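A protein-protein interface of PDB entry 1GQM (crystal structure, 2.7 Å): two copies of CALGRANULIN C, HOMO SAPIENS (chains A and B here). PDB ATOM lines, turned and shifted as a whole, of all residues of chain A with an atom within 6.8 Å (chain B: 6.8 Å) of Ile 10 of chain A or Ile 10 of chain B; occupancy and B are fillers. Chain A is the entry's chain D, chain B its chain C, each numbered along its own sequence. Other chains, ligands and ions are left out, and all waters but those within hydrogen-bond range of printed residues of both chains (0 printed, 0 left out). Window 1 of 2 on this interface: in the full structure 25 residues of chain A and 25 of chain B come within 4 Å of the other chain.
A ring nitrogen (ND1) of His 6 of chain B sits at hydrogen-bond distance from a ring nitrogen (ND1) of His 6 of chain A (2.8 Å).
Ile 13 of chain B touches Leu 3 of chain A.
His 6 of chain A touches Gly 9 of chain B (NE2 to CA, 3.5 Å).
CA of Gly 9 of chain A touches NE2 of His 6 of chain B, 3.6 Å away.
Ile 10 of chain A touches Leu 3 of chain B.
Ile 10 of chain A touches Leu 7 of chain B (CD1 to CD2, 3.6 Å).
CD1 of Ile 10 of chain A touches CD1 of Ile 10 of chain B (3.8 Å).
N of Leu 3 of chain B touches CD1 of Ile 13 of chain A, at 3.8 Å.
His 6 of chain B touches Ile 13 of chain A (CD2 to CD1, 3.8 Å).
Phe 70 of chain A touches Leu 81 of chain B (CE2 to O, 3.4 Å).
Ile 10 of chain B touches Leu 81 of chain A.
Printed residues of chain B within 4 Å of Leu 3 of chain A: Ile 13.
Printed residues of chain B within 4 Å of His 6 of chain A: His 6 (2.8 Å), Gly 9 (3.5 Å) and Ile 13 (3.9 Å).
Of the printed residues of chain B, Gly 9 of chain A touches His 6 (3.6 Å).
Ile 10 of chain A touches just these residues of chain B: Leu 3, Leu 7 and Ile 10.
Phe 73 of chain A touches none of the printed residues of chain B.
Printed residues of chain B within 4 Å of Val 77 of chain A: Leu 81.
Of chain A, only Ile 10 (3.8 Å) and Leu 81 (3.9 Å) come within 4 Å of Ile 10 of chain B.
Of the printed residues of chain A, Ile 13 of chain B touches Leu 3 (3.9 Å) and His 6 (3.9 Å).
The nearest residue of chain A that does not touch Ile 10 of chain B is His 6 of chain A (4.1 Å).
Printed residues of chain B that touch a printed residue of chain A: Leu 3, His 6, Leu 7, Gly 9, Ile 10, Val 11, Ile 13, Phe 70, Val 77 and Leu 81.
Hydrophobic or aromatic side chains of chain B that line the printed part of chain A: Leu 3, His 6, Leu 7, Ile 10, Val 11, Ile 13, Phe 70, Val 77 and Leu 81.
Among the printed residues, no Asp or Glu carboxylate lies within 4 Å of a Lys or Arg side-chain nitrogen of the other chain.
Ile 10 of chain A touches Leu 3 of chain B, but with the chains exchanged Leu 3 of chain A does not touch Ile 10 of chain B (4.2 Å).
Ile 10 of chain A touches Leu 7 of chain B, but with the chains exchanged Leu 7 of chain A does not touch Ile 10 of chain B (4.2 Å).
Ile 10 of chain B touches its own counterpart, Ile 10 of chain A.
Leu 81 of chain A touches Val 11 of chain B, but with the chains exchanged Val 11 of chain A does not touch Leu 81 of chain B (4.1 Å).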
ATOM      1  N   LEU A   3      -4.751 -22.799  10.723  1.00  0.00           N
ATOM      2  CA  LEU A   3      -4.969 -23.254  12.091  1.00  0.00           C
ATOM      3  C   LEU A   3      -4.312 -22.261  13.041  1.00  0.00           C
ATOM      4  O   LEU A   3      -4.916 -21.829  14.021  1.00  0.00           O
ATOM      5  CB  LEU A   3      -4.473 -24.690  12.286  1.00  0.00           C
ATOM      6  CG  LEU A   3      -4.872 -25.545  13.517  1.00  0.00           C
ATOM      7  CD1 LEU A   3      -4.535 -24.901  14.866  1.00  0.00           C
ATOM      8  CD2 LEU A   3      -6.331 -25.908  13.524  1.00  0.00           C
ATOM      9  N   GLU A   4      -3.083 -21.871  12.739  1.00  0.00           N
ATOM     10  CA  GLU A   4      -2.413 -20.866  13.549  1.00  0.00           C
ATOM     11  C   GLU A   4      -3.255 -19.594  13.557  1.00  0.00           C
ATOM     12  O   GLU A   4      -3.465 -18.993  14.604  1.00  0.00           O
ATOM     13  CB  GLU A   4      -1.007 -20.592  13.043  1.00  0.00           C
ATOM     14  CG  GLU A   4      -0.051 -21.731  13.335  1.00  0.00           C
ATOM     15  CD  GLU A   4       1.254 -21.656  12.532  1.00  0.00           C
ATOM     16  OE1 GLU A   4       1.338 -20.861  11.552  1.00  0.00           O
ATOM     17  OE2 GLU A   4       2.197 -22.412  12.886  1.00  0.00           O
ATOM     18  N   GLU A   5      -3.777 -19.218  12.392  1.00  0.00           N
ATOM     19  CA  GLU A   5      -4.582 -18.003  12.273  1.00  0.00           C
ATOM     20  C   GLU A   5      -5.854 -18.101  13.102  1.00  0.00           C
ATOM     21  O   GLU A   5      -6.243 -17.154  13.785  1.00  0.00           O
ATOM     22  CB  GLU A   5      -4.875 -17.642  10.804  1.00  0.00           C
ATOM     23  CG  GLU A   5      -3.674 -17.024  10.090  1.00  0.00           C
ATOM     24  CD  GLU A   5      -3.885 -16.800   8.581  1.00  0.00           C
ATOM     25  OE1 GLU A   5      -4.963 -16.276   8.199  1.00  0.00           O
ATOM     26  OE2 GLU A   5      -2.964 -17.121   7.764  1.00  0.00           O
ATOM     27  N   HIS A   6      -6.518 -19.239  13.060  1.00  0.00           N
ATOM     28  CA  HIS A   6      -7.655 -19.381  13.951  1.00  0.00           C
ATOM     29  C   HIS A   6      -7.238 -19.287  15.427  1.00  0.00           C
ATOM     30  O   HIS A   6      -7.957 -18.692  16.230  1.00  0.00           O
ATOM     31  CB  HIS A   6      -8.430 -20.651  13.659  1.00  0.00           C
ATOM     32  CG  HIS A   6      -9.164 -20.621  12.358  1.00  0.00           C
ATOM     33  ND1 HIS A   6     -10.107 -19.663  12.058  1.00  0.00           N
ATOM     34  CD2 HIS A   6      -9.099 -21.436  11.281  1.00  0.00           C
ATOM     35  CE1 HIS A   6     -10.587 -19.887  10.847  1.00  0.00           C
ATOM     36  NE2 HIS A   6      -9.991 -20.955  10.354  1.00  0.00           N
ATOM     37  N   LEU A   7      -6.078 -19.838  15.782  1.00  0.00           N
ATOM     38  CA  LEU A   7      -5.593 -19.735  17.172  1.00  0.00           C
ATOM     39  C   LEU A   7      -5.290 -18.291  17.576  1.00  0.00           C
ATOM     40  O   LEU A   7      -5.732 -17.806  18.594  1.00  0.00           O
ATOM     41  CB  LEU A   7      -4.386 -20.652  17.406  1.00  0.00           C
ATOM     42  CG  LEU A   7      -4.755 -22.147  17.254  1.00  0.00           C
ATOM     43  CD1 LEU A   7      -3.605 -23.061  17.548  1.00  0.00           C
ATOM     44  CD2 LEU A   7      -6.006 -22.551  18.067  1.00  0.00           C
ATOM     45  N   GLU A   8      -4.565 -17.566  16.741  1.00  0.00           N
ATOM     46  CA  GLU A   8      -4.299 -16.179  17.080  1.00  0.00           C
ATOM     47  C   GLU A   8      -5.641 -15.462  17.134  1.00  0.00           C
ATOM     48  O   GLU A   8      -5.847 -14.580  17.946  1.00  0.00           O
ATOM     49  CB  GLU A   8      -3.375 -15.555  16.074  1.00  0.00           C
ATOM     50  CG  GLU A   8      -2.493 -14.411  16.556  1.00  0.00           C
ATOM     51  CD  GLU A   8      -1.862 -13.659  15.345  1.00  0.00           C
ATOM     52  OE1 GLU A   8      -2.468 -13.688  14.223  1.00  0.00           O
ATOM     53  OE2 GLU A   8      -0.756 -13.051  15.484  1.00  0.00           O
ATOM     54  N   GLY A   9      -6.585 -15.869  16.300  1.00  0.00           N
ATOM     55  CA  GLY A   9      -7.903 -15.273  16.341  1.00  0.00           C
ATOM     56  C   GLY A   9      -8.519 -15.348  17.727  1.00  0.00           C
ATOM     57  O   GLY A   9      -8.971 -14.334  18.306  1.00  0.00           O
ATOM     58  N   ILE A  10      -8.523 -16.556  18.282  1.00  0.00           N
ATOM     59  CA  ILE A  10      -9.171 -16.750  19.540  1.00  0.00           C
ATOM     60  C   ILE A  10      -8.468 -15.895  20.548  1.00  0.00           C
ATOM     61  O   ILE A  10      -9.107 -15.302  21.417  1.00  0.00           O
ATOM     62  CB  ILE A  10      -9.168 -18.254  19.932  1.00  0.00           C
ATOM     63  CG1 ILE A  10     -10.215 -19.010  19.095  1.00  0.00           C
ATOM     64  CG2 ILE A  10      -9.467 -18.462  21.433  1.00  0.00           C
ATOM     65  CD1 ILE A  10     -10.140 -20.490  19.285  1.00  0.00           C
ATOM     66  N   VAL A  11      -7.155 -15.785  20.414  1.00  0.00           N
ATOM     67  CA  VAL A  11      -6.389 -15.040  21.398  1.00  0.00           C
ATOM     68  C   VAL A  11      -6.742 -13.572  21.290  1.00  0.00           C
ATOM     69  O   VAL A  11      -7.022 -12.903  22.298  1.00  0.00           O
ATOM     70  CB  VAL A  11      -4.881 -15.321  21.262  1.00  0.00           C
ATOM     71  CG1 VAL A  11      -4.050 -14.289  22.011  1.00  0.00           C
ATOM     72  CG2 VAL A  11      -4.600 -16.683  21.812  1.00  0.00           C
ATOM     73  N   ASN A  12      -6.771 -13.089  20.046  1.00  0.00           N
ATOM     74  CA  ASN A  12      -7.179 -11.716  19.761  1.00  0.00           C
ATOM     75  C   ASN A  12      -8.566 -11.415  20.344  1.00  0.00           C
ATOM     76  O   ASN A  12      -8.768 -10.404  20.994  1.00  0.00           O
ATOM     77  CB  ASN A  12      -7.074 -11.417  18.256  1.00  0.00           C
ATOM     78  CG  ASN A  12      -5.585 -11.283  17.771  1.00  0.00           C
ATOM     79  OD1 ASN A  12      -4.651 -11.132  18.602  1.00  0.00           O
ATOM     80  ND2 ASN A  12      -5.364 -11.359  16.435  1.00  0.00           N
ATOM     81  N   ILE A  13      -9.509 -12.329  20.202  1.00  0.00           N
ATOM     82  CA  ILE A  13     -10.821 -12.000  20.696  1.00  0.00           C
ATOM     83  C   ILE A  13     -10.828 -11.909  22.199  1.00  0.00           C
ATOM     84  O   ILE A  13     -11.504 -11.077  22.777  1.00  0.00           O
ATOM     85  CB  ILE A  13     -11.838 -12.949  20.127  1.00  0.00           C
ATOM     86  CG1 ILE A  13     -11.974 -12.616  18.641  1.00  0.00           C
ATOM     87  CG2 ILE A  13     -13.177 -12.792  20.810  1.00  0.00           C
ATOM     88  CD1 ILE A  13     -12.597 -13.693  17.824  1.00  0.00           C
ATOM     89  N   PHE A  14     -10.027 -12.730  22.838  1.00  0.00           N
ATOM     90  CA  PHE A  14      -9.929 -12.694  24.295  1.00  0.00           C
ATOM     91  C   PHE A  14      -9.581 -11.298  24.714  1.00  0.00           C
ATOM     92  O   PHE A  14     -10.294 -10.681  25.482  1.00  0.00           O
ATOM     93  CB  PHE A  14      -8.823 -13.639  24.765  1.00  0.00           C
ATOM     94  CG  PHE A  14      -8.701 -13.766  26.252  1.00  0.00           C
ATOM     95  CD1 PHE A  14      -9.661 -14.463  26.992  1.00  0.00           C
ATOM     96  CD2 PHE A  14      -7.603 -13.202  26.920  1.00  0.00           C
ATOM     97  CE1 PHE A  14      -9.508 -14.580  28.375  1.00  0.00           C
ATOM     98  CE2 PHE A  14      -7.445 -13.316  28.298  1.00  0.00           C
ATOM     99  CZ  PHE A  14      -8.375 -14.000  29.022  1.00  0.00           C
ATOM    100  N   HIS A  15      -8.481 -10.787  24.189  1.00  0.00           N
ATOM    101  CA  HIS A  15      -8.032  -9.459  24.584  1.00  0.00           C
ATOM    102  C   HIS A  15      -8.957  -8.378  24.176  1.00  0.00           C
ATOM    103  O   HIS A  15      -9.095  -7.374  24.841  1.00  0.00           O
ATOM    104  CB  HIS A  15      -6.630  -9.183  24.103  1.00  0.00           C
ATOM    105  CG  HIS A  15      -5.634 -10.008  24.830  1.00  0.00           C
ATOM    106  ND1 HIS A  15      -4.665 -10.751  24.197  1.00  0.00           N
ATOM    107  CD2 HIS A  15      -5.529 -10.290  26.145  1.00  0.00           C
ATOM    108  CE1 HIS A  15      -3.988 -11.440  25.097  1.00  0.00           C
ATOM    109  NE2 HIS A  15      -4.491 -11.176  26.286  1.00  0.00           N
ATOM    110  N   PHE A  70      -6.458 -16.125  31.034  1.00  0.00           N
ATOM    111  CA  PHE A  70      -6.348 -16.850  29.778  1.00  0.00           C
ATOM    112  C   PHE A  70      -6.325 -18.352  30.004  1.00  0.00           C
ATOM    113  O   PHE A  70      -6.977 -19.093  29.296  1.00  0.00           O
ATOM    114  CB  PHE A  70      -5.201 -16.333  28.843  1.00  0.00           C
ATOM    115  CG  PHE A  70      -5.219 -16.988  27.483  1.00  0.00           C
ATOM    116  CD1 PHE A  70      -6.146 -16.602  26.522  1.00  0.00           C
ATOM    117  CD2 PHE A  70      -4.397 -18.073  27.202  1.00  0.00           C
ATOM    118  CE1 PHE A  70      -6.229 -17.240  25.312  1.00  0.00           C
ATOM    119  CE2 PHE A  70      -4.479 -18.701  25.971  1.00  0.00           C
ATOM    120  CZ  PHE A  70      -5.388 -18.275  25.037  1.00  0.00           C
ATOM    121  N   PHE A  73      -9.649 -19.377  30.492  1.00  0.00           N
ATOM    122  CA  PHE A  73     -10.440 -19.169  29.325  1.00  0.00           C
ATOM    123  C   PHE A  73     -10.438 -20.424  28.483  1.00  0.00           C
ATOM    124  O   PHE A  73     -11.458 -20.818  27.914  1.00  0.00           O
ATOM    125  CB  PHE A  73      -9.877 -17.989  28.556  1.00  0.00           C
ATOM    126  CG  PHE A  73     -10.699 -17.579  27.370  1.00  0.00           C
ATOM    127  CD1 PHE A  73     -10.154 -17.581  26.105  1.00  0.00           C
ATOM    128  CD2 PHE A  73     -12.006 -17.192  27.522  1.00  0.00           C
ATOM    129  CE1 PHE A  73     -10.903 -17.202  25.024  1.00  0.00           C
ATOM    130  CE2 PHE A  73     -12.750 -16.800  26.428  1.00  0.00           C
ATOM    131  CZ  PHE A  73     -12.197 -16.798  25.189  1.00  0.00           C
ATOM    132  N   VAL A  77     -13.010 -22.593  25.650  1.00  0.00           N
ATOM    133  CA  VAL A  77     -12.841 -22.810  24.227  1.00  0.00           C
ATOM    134  C   VAL A  77     -13.173 -24.242  23.990  1.00  0.00           C
ATOM    135  O   VAL A  77     -13.776 -24.613  22.985  1.00  0.00           O
ATOM    136  CB  VAL A  77     -11.396 -22.568  23.722  1.00  0.00           C
ATOM    137  CG1 VAL A  77     -11.223 -23.209  22.365  1.00  0.00           C
ATOM    138  CG2 VAL A  77     -11.134 -21.118  23.574  1.00  0.00           C
ATOM    139  N   LEU A  81     -15.916 -25.584  21.550  1.00  0.00           N
ATOM    140  CA  LEU A  81     -15.440 -26.345  20.432  1.00  0.00           C
ATOM    141  C   LEU A  81     -16.243 -27.617  20.398  1.00  0.00           C
ATOM    142  O   LEU A  81     -16.425 -28.252  19.344  1.00  0.00           O
ATOM    143  CB  LEU A  81     -13.972 -26.666  20.614  1.00  0.00           C
ATOM    144  CG  LEU A  81     -13.187 -26.463  19.328  1.00  0.00           C
ATOM    145  CD1 LEU A  81     -11.743 -26.847  19.603  1.00  0.00           C
ATOM    146  CD2 LEU A  81     -13.766 -27.336  18.238  1.00  0.00           C
ATOM    147  N   LEU B   3     -15.857 -15.364  16.833  1.00  0.00           N
ATOM    148  CA  LEU B   3     -15.392 -16.522  17.638  1.00  0.00           C
ATOM    149  C   LEU B   3     -15.910 -17.817  17.066  1.00  0.00           C
ATOM    150  O   LEU B   3     -15.179 -18.773  16.944  1.00  0.00           O
ATOM    151  CB  LEU B   3     -15.803 -16.449  19.111  1.00  0.00           C
ATOM    152  CG  LEU B   3     -14.782 -16.968  20.125  1.00  0.00           C
ATOM    153  CD1 LEU B   3     -15.403 -17.771  21.239  1.00  0.00           C
ATOM    154  CD2 LEU B   3     -13.701 -17.814  19.507  1.00  0.00           C
ATOM    155  N   GLU B   5     -16.910 -18.304  14.078  1.00  0.00           N
ATOM    156  CA  GLU B   5     -16.192 -18.536  12.836  1.00  0.00           C
ATOM    157  C   GLU B   5     -14.921 -19.366  13.114  1.00  0.00           C
ATOM    158  O   GLU B   5     -14.717 -20.428  12.540  1.00  0.00           O
ATOM    159  N   HIS B   6     -14.080 -18.892  14.017  1.00  0.00           N
ATOM    160  CA  HIS B   6     -12.820 -19.568  14.297  1.00  0.00           C
ATOM    161  C   HIS B   6     -13.000 -21.009  14.746  1.00  0.00           C
ATOM    162  O   HIS B   6     -12.322 -21.941  14.276  1.00  0.00           O
ATOM    163  CB  HIS B   6     -12.022 -18.759  15.310  1.00  0.00           C
ATOM    164  CG  HIS B   6     -11.466 -17.496  14.733  1.00  0.00           C
ATOM    165  ND1 HIS B   6     -10.920 -17.443  13.464  1.00  0.00           N
ATOM    166  CD2 HIS B   6     -11.387 -16.242  15.233  1.00  0.00           C
ATOM    167  CE1 HIS B   6     -10.534 -16.207  13.212  1.00  0.00           C
ATOM    168  NE2 HIS B   6     -10.809 -15.458  14.265  1.00  0.00           N
ATOM    169  N   LEU B   7     -13.931 -21.187  15.662  1.00  0.00           N
ATOM    170  CA  LEU B   7     -14.202 -22.515  16.129  1.00  0.00           C
ATOM    171  C   LEU B   7     -14.637 -23.380  14.937  1.00  0.00           C
ATOM    172  O   LEU B   7     -14.165 -24.514  14.781  1.00  0.00           O
ATOM    173  CB  LEU B   7     -15.226 -22.474  17.248  1.00  0.00           C
ATOM    174  CG  LEU B   7     -14.776 -21.632  18.442  1.00  0.00           C
ATOM    175  CD1 LEU B   7     -15.769 -21.754  19.581  1.00  0.00           C
ATOM    176  CD2 LEU B   7     -13.415 -22.028  18.874  1.00  0.00           C
ATOM    177  N   GLU B   8     -15.490 -22.838  14.061  1.00  0.00           N
ATOM    178  CA  GLU B   8     -15.895 -23.625  12.901  1.00  0.00           C
ATOM    179  C   GLU B   8     -14.711 -23.921  12.006  1.00  0.00           C
ATOM    180  O   GLU B   8     -14.606 -24.994  11.433  1.00  0.00           O
ATOM    181  CB  GLU B   8     -17.050 -23.013  12.126  1.00  0.00           C
ATOM    182  CG  GLU B   8     -17.840 -24.110  11.427  1.00  0.00           C
ATOM    183  CD  GLU B   8     -19.100 -23.646  10.726  1.00  0.00           C
ATOM    184  OE1 GLU B   8     -19.239 -22.424  10.446  1.00  0.00           O
ATOM    185  OE2 GLU B   8     -19.954 -24.524  10.441  1.00  0.00           O
ATOM    186  N   GLY B   9     -13.800 -22.971  11.913  1.00  0.00           N
ATOM    187  CA  GLY B   9     -12.562 -23.208  11.212  1.00  0.00           C
ATOM    188  C   GLY B   9     -11.833 -24.425  11.756  1.00  0.00           C
ATOM    189  O   GLY B   9     -11.536 -25.357  11.014  1.00  0.00           O
ATOM    190  N   ILE B  10     -11.566 -24.423  13.061  1.00  0.00           N
ATOM    191  CA  ILE B  10     -10.851 -25.516  13.713  1.00  0.00           C
ATOM    192  C   ILE B  10     -11.527 -26.861  13.396  1.00  0.00           C
ATOM    193  O   ILE B  10     -10.885 -27.809  12.944  1.00  0.00           O
ATOM    194  CB  ILE B  10     -10.695 -25.217  15.249  1.00  0.00           C
ATOM    195  CG1 ILE B  10      -9.604 -24.174  15.483  1.00  0.00           C
ATOM    196  CG2 ILE B  10     -10.285 -26.439  15.999  1.00  0.00           C
ATOM    197  CD1 ILE B  10      -9.890 -23.174  16.543  1.00  0.00           C
ATOM    198  N   VAL B  11     -12.838 -26.915  13.553  1.00  0.00           N
ATOM    199  CA  VAL B  11     -13.556 -28.128  13.223  1.00  0.00           C
ATOM    200  C   VAL B  11     -13.283 -28.522  11.787  1.00  0.00           C
ATOM    201  O   VAL B  11     -12.944 -29.663  11.498  1.00  0.00           O
ATOM    202  CB  VAL B  11     -15.052 -27.914  13.355  1.00  0.00           C
ATOM    203  CG1 VAL B  11     -15.806 -29.044  12.725  1.00  0.00           C
ATOM    204  CG2 VAL B  11     -15.434 -27.810  14.769  1.00  0.00           C
ATOM    205  N   ASN B  12     -13.447 -27.568  10.876  1.00  0.00           N
ATOM    206  CA  ASN B  12     -13.231 -27.874   9.484  1.00  0.00           C
ATOM    207  C   ASN B  12     -11.779 -28.371   9.259  1.00  0.00           C
ATOM    208  O   ASN B  12     -11.575 -29.324   8.509  1.00  0.00           O
ATOM    209  CB  ASN B  12     -13.624 -26.701   8.579  1.00  0.00           C
ATOM    210  CG  ASN B  12     -15.182 -26.397   8.558  1.00  0.00           C
ATOM    211  OD1 ASN B  12     -16.032 -27.292   8.607  1.00  0.00           O
ATOM    212  ND2 ASN B  12     -15.520 -25.114   8.440  1.00  0.00           N
ATOM    213  N   ILE B  13     -10.771 -27.801   9.931  1.00  0.00           N
ATOM    214  CA  ILE B  13      -9.420 -28.310   9.685  1.00  0.00           C
ATOM    215  C   ILE B  13      -9.330 -29.757  10.112  1.00  0.00           C
ATOM    216  O   ILE B  13      -8.738 -30.603   9.430  1.00  0.00           O
ATOM    217  CB  ILE B  13      -8.296 -27.518  10.363  1.00  0.00           C
ATOM    218  CG1 ILE B  13      -7.911 -26.304   9.550  1.00  0.00           C
ATOM    219  CG2 ILE B  13      -7.047 -28.326  10.354  1.00  0.00           C
ATOM    220  CD1 ILE B  13      -8.249 -25.094  10.187  1.00  0.00           C
ATOM    221  N   PHE B  14      -9.912 -30.064  11.257  1.00  0.00           N
ATOM    222  CA  PHE B  14      -9.857 -31.446  11.720  1.00  0.00           C
ATOM    223  C   PHE B  14     -10.247 -32.345  10.559  1.00  0.00           C
ATOM    224  O   PHE B  14      -9.479 -33.220  10.120  1.00  0.00           O
ATOM    225  CB  PHE B  14     -10.857 -31.649  12.828  1.00  0.00           C
ATOM    226  CG  PHE B  14     -10.859 -33.027  13.424  1.00  0.00           C
ATOM    227  CD1 PHE B  14      -9.807 -33.454  14.218  1.00  0.00           C
ATOM    228  CD2 PHE B  14     -11.965 -33.858  13.267  1.00  0.00           C
ATOM    229  CE1 PHE B  14      -9.832 -34.699  14.788  1.00  0.00           C
ATOM    230  CE2 PHE B  14     -12.008 -35.105  13.848  1.00  0.00           C
ATOM    231  CZ  PHE B  14     -10.945 -35.532  14.610  1.00  0.00           C
ATOM    232  N   HIS B  15     -11.450 -32.098  10.044  1.00  0.00           N
ATOM    233  CA  HIS B  15     -12.000 -32.932   9.016  1.00  0.00           C
ATOM    234  C   HIS B  15     -11.171 -32.851   7.749  1.00  0.00           C
ATOM    235  O   HIS B  15     -11.038 -33.838   7.013  1.00  0.00           O
ATOM    236  CB  HIS B  15     -13.473 -32.623   8.794  1.00  0.00           C
ATOM    237  CG  HIS B  15     -14.361 -33.156   9.874  1.00  0.00           C
ATOM    238  ND1 HIS B  15     -15.402 -32.429  10.416  1.00  0.00           N
ATOM    239  CD2 HIS B  15     -14.360 -34.349  10.523  1.00  0.00           C
ATOM    240  CE1 HIS B  15     -16.002 -33.147  11.352  1.00  0.00           C
ATOM    241  NE2 HIS B  15     -15.390 -34.318  11.437  1.00  0.00           N
ATOM    242  N   GLN B  16     -10.563 -31.706   7.491  1.00  0.00           N
ATOM    243  CA  GLN B  16      -9.701 -31.641   6.319  1.00  0.00           C
ATOM    244  C   GLN B  16      -8.671 -32.789   6.420  1.00  0.00           C
ATOM    245  O   GLN B  16      -8.310 -33.392   5.441  1.00  0.00           O
ATOM    246  CB  GLN B  16      -9.016 -30.257   6.217  1.00  0.00           C
ATOM    247  CG  GLN B  16      -8.293 -29.959   4.879  1.00  0.00           C
ATOM    248  CD  GLN B  16      -7.397 -28.684   4.924  1.00  0.00           C
ATOM    249  OE1 GLN B  16      -7.833 -27.605   5.384  1.00  0.00           O
ATOM    250  NE2 GLN B  16      -6.157 -28.811   4.435  1.00  0.00           N
ATOM    251  N   LEU B  35      -1.392 -33.027   9.707  1.00  0.00           N
ATOM    252  CA  LEU B  35      -1.955 -31.898  10.431  1.00  0.00           C
ATOM    253  C   LEU B  35      -0.911 -31.154  11.291  1.00  0.00           C
ATOM    254  O   LEU B  35      -0.763 -29.934  11.206  1.00  0.00           O
ATOM    255  CB  LEU B  35      -3.131 -32.353  11.290  1.00  0.00           C
ATOM    256  CG  LEU B  35      -3.881 -31.181  11.887  1.00  0.00           C
ATOM    257  CD1 LEU B  35      -5.332 -31.534  12.078  1.00  0.00           C
ATOM    258  CD2 LEU B  35      -3.237 -30.828  13.214  1.00  0.00           C
ATOM    259  N   PHE B  70     -12.351 -36.587  17.716  1.00  0.00           N
ATOM    260  CA  PHE B  70     -12.503 -35.163  17.953  1.00  0.00           C
ATOM    261  C   PHE B  70     -12.336 -34.828  19.403  1.00  0.00           C
ATOM    262  O   PHE B  70     -11.579 -33.926  19.722  1.00  0.00           O
ATOM    263  CB  PHE B  70     -13.788 -34.588  17.355  1.00  0.00           C
ATOM    264  CG  PHE B  70     -13.853 -33.088  17.434  1.00  0.00           C
ATOM    265  CD1 PHE B  70     -12.989 -32.305  16.693  1.00  0.00           C
ATOM    266  CD2 PHE B  70     -14.758 -32.455  18.268  1.00  0.00           C
ATOM    267  CE1 PHE B  70     -13.042 -30.916  16.791  1.00  0.00           C
ATOM    268  CE2 PHE B  70     -14.801 -31.093  18.369  1.00  0.00           C
ATOM    269  CZ  PHE B  70     -13.957 -30.313  17.634  1.00  0.00           C
ATOM    270  N   PHE B  73      -8.959 -34.677  20.199  1.00  0.00           N
ATOM    271  CA  PHE B  73      -8.270 -33.591  19.485  1.00  0.00           C
ATOM    272  C   PHE B  73      -8.370 -32.296  20.266  1.00  0.00           C
ATOM    273  O   PHE B  73      -7.414 -31.510  20.266  1.00  0.00           O
ATOM    274  CB  PHE B  73      -8.832 -33.459  18.062  1.00  0.00           C
ATOM    275  CG  PHE B  73      -8.210 -32.375  17.199  1.00  0.00           C
ATOM    276  CD1 PHE B  73      -8.956 -31.281  16.801  1.00  0.00           C
ATOM    277  CD2 PHE B  73      -6.943 -32.499  16.689  1.00  0.00           C
ATOM    278  CE1 PHE B  73      -8.423 -30.309  15.983  1.00  0.00           C
ATOM    279  CE2 PHE B  73      -6.402 -31.501  15.851  1.00  0.00           C
ATOM    280  CZ  PHE B  73      -7.150 -30.417  15.520  1.00  0.00           C
ATOM    281  N   VAL B  77      -5.954 -28.657  20.826  1.00  0.00           N
ATOM    282  CA  VAL B  77      -6.212 -27.255  20.690  1.00  0.00           C
ATOM    283  C   VAL B  77      -5.727 -26.608  21.973  1.00  0.00           C
ATOM    284  O   VAL B  77      -5.052 -25.614  21.960  1.00  0.00           O
ATOM    285  CB  VAL B  77      -7.675 -26.969  20.490  1.00  0.00           C
ATOM    286  CG1 VAL B  77      -7.949 -25.519  20.751  1.00  0.00           C
ATOM    287  CG2 VAL B  77      -8.054 -27.268  19.093  1.00  0.00           C
ATOM    288  N   LEU B  81      -3.333 -23.501  21.883  1.00  0.00           N
ATOM    289  CA  LEU B  81      -3.832 -22.220  22.324  1.00  0.00           C
ATOM    290  C   LEU B  81      -2.931 -21.621  23.372  1.00  0.00           C
ATOM    291  O   LEU B  81      -2.829 -20.392  23.516  1.00  0.00           O
ATOM    292  CB  LEU B  81      -5.159 -22.439  23.001  1.00  0.00           C
ATOM    293  CG  LEU B  81      -6.257 -22.011  22.090  1.00  0.00           C
ATOM    294  CD1 LEU B  81      -7.582 -22.274  22.810  1.00  0.00           C
ATOM    295  CD2 LEU B  81      -6.023 -20.523  21.803  1.00  0.00           C
